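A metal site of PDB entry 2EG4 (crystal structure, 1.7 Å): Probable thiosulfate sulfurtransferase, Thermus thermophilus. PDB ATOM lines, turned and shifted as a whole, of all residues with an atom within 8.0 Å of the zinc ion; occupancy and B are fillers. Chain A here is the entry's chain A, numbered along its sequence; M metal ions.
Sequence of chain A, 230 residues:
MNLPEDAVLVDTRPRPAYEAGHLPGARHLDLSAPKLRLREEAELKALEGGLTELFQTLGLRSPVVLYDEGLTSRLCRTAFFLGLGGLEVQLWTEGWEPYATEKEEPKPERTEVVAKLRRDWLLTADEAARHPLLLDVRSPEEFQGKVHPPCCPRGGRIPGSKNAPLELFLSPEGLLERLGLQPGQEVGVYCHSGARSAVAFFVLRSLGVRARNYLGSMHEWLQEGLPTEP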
ATOM      1  N   LYS A  35      25.786  15.041  -8.565  1.00  0.00           N
ATOM      2  CA  LYS A  35      25.004  14.253  -7.604  1.00  0.00           C
ATOM      3  C   LYS A  35      23.852  15.197  -7.221  1.00  0.00           C
ATOM      4  O   LYS A  35      24.070  16.343  -6.845  1.00  0.00           O
ATOM      5  CB  LYS A  35      25.847  13.880  -6.376  1.00  0.00           C
ATOM      6  CG  LYS A  35      26.676  12.606  -6.590  1.00  0.00           C
ATOM      7  CD  LYS A  35      27.373  12.177  -5.307  1.00  0.00           C
ATOM      8  CE  LYS A  35      28.593  13.020  -5.032  1.00  0.00           C
ATOM      9  NZ  LYS A  35      29.685  12.667  -5.983  1.00  0.00           N
ATOM     10  N   HIS A 148      31.215   0.683   0.513  1.00  0.00           N
ATOM     11  CA  HIS A 148      30.490   1.885   0.153  1.00  0.00           C
ATOM     12  C   HIS A 148      31.491   2.914  -0.351  1.00  0.00           C
ATOM     13  O   HIS A 148      32.664   2.883   0.044  1.00  0.00           O
ATOM     14  CB  HIS A 148      29.748   2.470   1.359  1.00  0.00           C
ATOM     15  CG  HIS A 148      30.640   2.858   2.488  1.00  0.00           C
ATOM     16  ND1 HIS A 148      31.184   1.931   3.358  1.00  0.00           N
ATOM     17  CD2 HIS A 148      31.124   4.060   2.868  1.00  0.00           C
ATOM     18  CE1 HIS A 148      31.956   2.554   4.227  1.00  0.00           C
ATOM     19  NE2 HIS A 148      31.937   3.845   3.962  1.00  0.00           N
ATOM     20  N   PRO A 149      31.062   3.819  -1.234  1.00  0.00           N
ATOM     21  CA  PRO A 149      31.999   4.826  -1.733  1.00  0.00           C
ATOM     22  C   PRO A 149      32.392   5.775  -0.599  1.00  0.00           C
ATOM     23  O   PRO A 149      31.610   6.004   0.329  1.00  0.00           O
ATOM     24  CB  PRO A 149      31.217   5.496  -2.862  1.00  0.00           C
ATOM     25  CG  PRO A 149      29.788   5.348  -2.417  1.00  0.00           C
ATOM     26  CD  PRO A 149      29.751   3.928  -1.898  1.00  0.00           C
ATOM     27  N   PRO A 150      33.619   6.327  -0.647  1.00  0.00           N
ATOM     28  CA  PRO A 150      34.129   7.247   0.376  1.00  0.00           C
ATOM     29  C   PRO A 150      33.335   8.531   0.606  1.00  0.00           C
ATOM     30  O   PRO A 150      33.441   9.149   1.661  1.00  0.00           O
ATOM     31  CB  PRO A 150      35.565   7.511  -0.085  1.00  0.00           C
ATOM     32  CG  PRO A 150      35.476   7.393  -1.568  1.00  0.00           C
ATOM     33  CD  PRO A 150      34.596   6.164  -1.740  1.00  0.00           C
ATOM     34  N   CYS A 151      32.537   8.924  -0.385  1.00  0.00           N
ATOM     35  CA  CYS A 151      31.726  10.128  -0.240  1.00  0.00           C
ATOM     36  C   CYS A 151      30.502   9.864   0.651  1.00  0.00           C
ATOM     37  O   CYS A 151      29.784  10.785   1.023  1.00  0.00           O
ATOM     38  CB  CYS A 151      31.273  10.605  -1.612  1.00  0.00           C
ATOM     39  SG  CYS A 151      30.392   9.328  -2.542  1.00  0.00           S
ATOM     40  N   CYS A 152      30.263   8.595   0.992  1.00  0.00           N
ATOM     41  CA  CYS A 152      29.103   8.241   1.829  1.00  0.00           C
ATOM     42  C   CYS A 152      29.508   7.854   3.272  1.00  0.00           C
ATOM     43  O   CYS A 152      30.639   7.444   3.505  1.00  0.00           O
ATOM     44  CB  CYS A 152      28.297   7.107   1.189  1.00  0.00           C
ATOM     45  SG  CYS A 152      27.145   7.607  -0.168  1.00  0.00           S
ATOM     46  N   PRO A 153      28.585   7.966   4.235  1.00  0.00           N
ATOM     47  CA  PRO A 153      28.838   7.635   5.651  1.00  0.00           C
ATOM     48  C   PRO A 153      29.104   6.179   6.006  1.00  0.00           C
ATOM     49  O   PRO A 153      29.924   5.889   6.884  1.00  0.00           O
ATOM     50  CB  PRO A 153      27.584   8.137   6.363  1.00  0.00           C
ATOM     51  CG  PRO A 153      27.085   9.215   5.496  1.00  0.00           C
ATOM     52  CD  PRO A 153      27.304   8.675   4.109  1.00  0.00           C
ATOM     53  N   ARG A 154      28.418   5.254   5.340  1.00  0.00           N
ATOM     54  CA  ARG A 154      28.571   3.835   5.646  1.00  0.00           C
ATOM     55  C   ARG A 154      27.944   2.960   4.576  1.00  0.00           C
ATOM     56  O   ARG A 154      27.390   3.464   3.602  1.00  0.00           O
ATOM     57  CB  ARG A 154      27.903   3.540   6.982  1.00  0.00           C
ATOM     58  CG  ARG A 154      26.478   4.053   7.023  1.00  0.00           C
ATOM     59  CD  ARG A 154      25.850   3.902   8.403  1.00  0.00           C
ATOM     60  NE  ARG A 154      24.532   4.532   8.459  1.00  0.00           N
ATOM     61  CZ  ARG A 154      23.540   4.248   7.627  1.00  0.00           C
ATOM     62  NH1 ARG A 154      23.727   3.342   6.668  1.00  0.00           N
ATOM     63  NH2 ARG A 154      22.373   4.856   7.740  1.00  0.00           N
ATOM     64  N   HIS A 192      24.104   4.152  -6.479  1.00  0.00           N
ATOM     65  CA  HIS A 192      24.768   5.195  -5.696  1.00  0.00           C
ATOM     66  C   HIS A 192      24.319   6.585  -6.106  1.00  0.00           C
ATOM     67  O   HIS A 192      23.912   7.387  -5.270  1.00  0.00           O
ATOM     68  CB  HIS A 192      26.294   5.114  -5.836  1.00  0.00           C
ATOM     69  CG  HIS A 192      27.019   6.185  -5.078  1.00  0.00           C
ATOM     70  ND1 HIS A 192      27.880   7.067  -5.680  1.00  0.00           N
ATOM     71  CD2 HIS A 192      26.956   6.547  -3.767  1.00  0.00           C
ATOM     72  CE1 HIS A 192      28.319   7.935  -4.789  1.00  0.00           C
ATOM     73  NE2 HIS A 192      27.776   7.642  -3.627  1.00  0.00           N
ATOM     74  N   SER A 193      24.379   6.901  -7.401  1.00  0.00           N
ATOM     75  CA  SER A 193      23.938   8.204  -7.821  1.00  0.00           C
ATOM     76  C   SER A 193      23.125   8.127  -9.099  1.00  0.00           C
ATOM     77  O   SER A 193      23.108   9.057  -9.903  1.00  0.00           O
ATOM     78  CB  SER A 193      25.105   9.190  -7.992  1.00  0.00           C
ATOM     79  OG  SER A 193      26.021   8.767  -9.010  1.00  0.00           O
ATOM     80  N   GLY A 216      18.466  10.370  -6.992  1.00  0.00           N
ATOM     81  CA  GLY A 216      19.245  10.705  -5.808  1.00  0.00           C
ATOM     82  C   GLY A 216      20.008   9.500  -5.308  1.00  0.00           C
ATOM     83  O   GLY A 216      21.179   9.577  -4.831  1.00  0.00           O
ATOM     84  N   MET A 218      21.332   6.057  -3.331  1.00  0.00           N
ATOM     85  CA  MET A 218      21.911   5.869  -1.997  1.00  0.00           C
ATOM     86  C   MET A 218      22.698   7.072  -1.432  1.00  0.00           C
ATOM     87  O   MET A 218      22.695   7.316  -0.226  1.00  0.00           O
ATOM     88  CB  MET A 218      22.798   4.608  -1.998  1.00  0.00           C
ATOM     89  CG  MET A 218      22.756   3.806  -0.705  1.00  0.00           C
ATOM     90  SD  MET A 218      21.078   3.181  -0.254  1.00  0.00           S
ATOM     91  CE  MET A 218      21.279   3.183   1.505  1.00  0.00           C
ATOM     92  N   HIS A 219      23.373   7.826  -2.290  1.00  0.00           N
ATOM     93  CA  HIS A 219      24.085   8.995  -1.789  1.00  0.00           C
ATOM     94  C   HIS A 219      23.088   9.949  -1.129  1.00  0.00           C
ATOM     95  O   HIS A 219      23.278  10.355   0.024  1.00  0.00           O
ATOM     96  CB  HIS A 219      24.850   9.710  -2.912  1.00  0.00           C
ATOM     97  CG  HIS A 219      25.747  10.806  -2.419  1.00  0.00           C
ATOM     98  ND1 HIS A 219      27.049  10.582  -2.033  1.00  0.00           N
ATOM     99  CD2 HIS A 219      25.514  12.124  -2.215  1.00  0.00           C
ATOM    100  CE1 HIS A 219      27.577  11.715  -1.607  1.00  0.00           C
ATOM    101  NE2 HIS A 219      26.671  12.667  -1.711  1.00  0.00           N
ATOM    102  N   GLU A 220      22.019  10.294  -1.827  1.00  0.00           N
ATOM    103  CA  GLU A 220      21.048  11.211  -1.250  1.00  0.00           C
ATOM    104  C   GLU A 220      20.380  10.598  -0.030  1.00  0.00           C
ATOM    105  O   GLU A 220      20.227  11.243   0.998  1.00  0.00           O
ATOM    106  CB  GLU A 220      19.962  11.571  -2.240  1.00  0.00           C
ATOM    107  CG  GLU A 220      18.917  12.468  -1.614  1.00  0.00           C
ATOM    108  CD  GLU A 220      17.736  12.699  -2.514  1.00  0.00           C
ATOM    109  OE1 GLU A 220      17.244  11.710  -3.110  1.00  0.00           O
ATOM    110  OE2 GLU A 220      17.282  13.859  -2.593  1.00  0.00           O
ATOM    111  N   LEU A 222      21.425   8.545   2.178  1.00  0.00           N
ATOM    112  CA  LEU A 222      22.258   8.640   3.376  1.00  0.00           C
ATOM    113  C   LEU A 222      22.441  10.094   3.828  1.00  0.00           C
ATOM    114  O   LEU A 222      22.435  10.364   5.024  1.00  0.00           O
ATOM    115  CB  LEU A 222      23.625   7.994   3.126  1.00  0.00           C
ATOM    116  CG  LEU A 222      23.592   6.461   2.995  1.00  0.00           C
ATOM    117  CD1 LEU A 222      24.973   5.934   2.614  1.00  0.00           C
ATOM    118  CD2 LEU A 222      23.129   5.849   4.337  1.00  0.00           C
ATOM    119  N   GLN A 223      22.598  11.018   2.896  1.00  0.00           N
ATOM    120  CA  GLN A 223      22.761  12.421   3.301  1.00  0.00           C
ATOM    121  C   GLN A 223      21.541  12.887   4.086  1.00  0.00           C
ATOM    122  O   GLN A 223      21.649  13.668   5.031  1.00  0.00           O
ATOM    123  CB  GLN A 223      22.977  13.306   2.070  1.00  0.00           C
ATOM    124  CG  GLN A 223      24.377  13.170   1.473  1.00  0.00           C
ATOM    125  CD  GLN A 223      25.474  13.400   2.507  1.00  0.00           C
ATOM    126  OE1 GLN A 223      25.452  14.388   3.254  1.00  0.00           O
ATOM    127  NE2 GLN A 223      26.448  12.490   2.560  1.00  0.00           N
HETATM  128 ZN    ZN M   1      28.188   8.779  -1.913  1.00  0.00          ZN
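Pro 149 touches the zinc ion (CG to ZN, 3.8 Å). Within 4 Å of the zinc ion: Pro 149, Cys 151, Cys 152, His 192 and His 219.
The zinc ion is bound by a ring nitrogen (NE2) of His 192 (2.1 Å), a ring nitrogen (ND1) of His 219 (2.1 Å), the side-chain sulfur of Cys 152 (2.3 Å) and the side-chain sulfur of Cys 151 (2.4 Å). The zinc ion has four donor atoms within binding distance.
The backbone carbonyl oxygen (O) of His 192 lies within hydrogen-bond range of the backbone NH (N) of Met 218 (3.5 Å).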
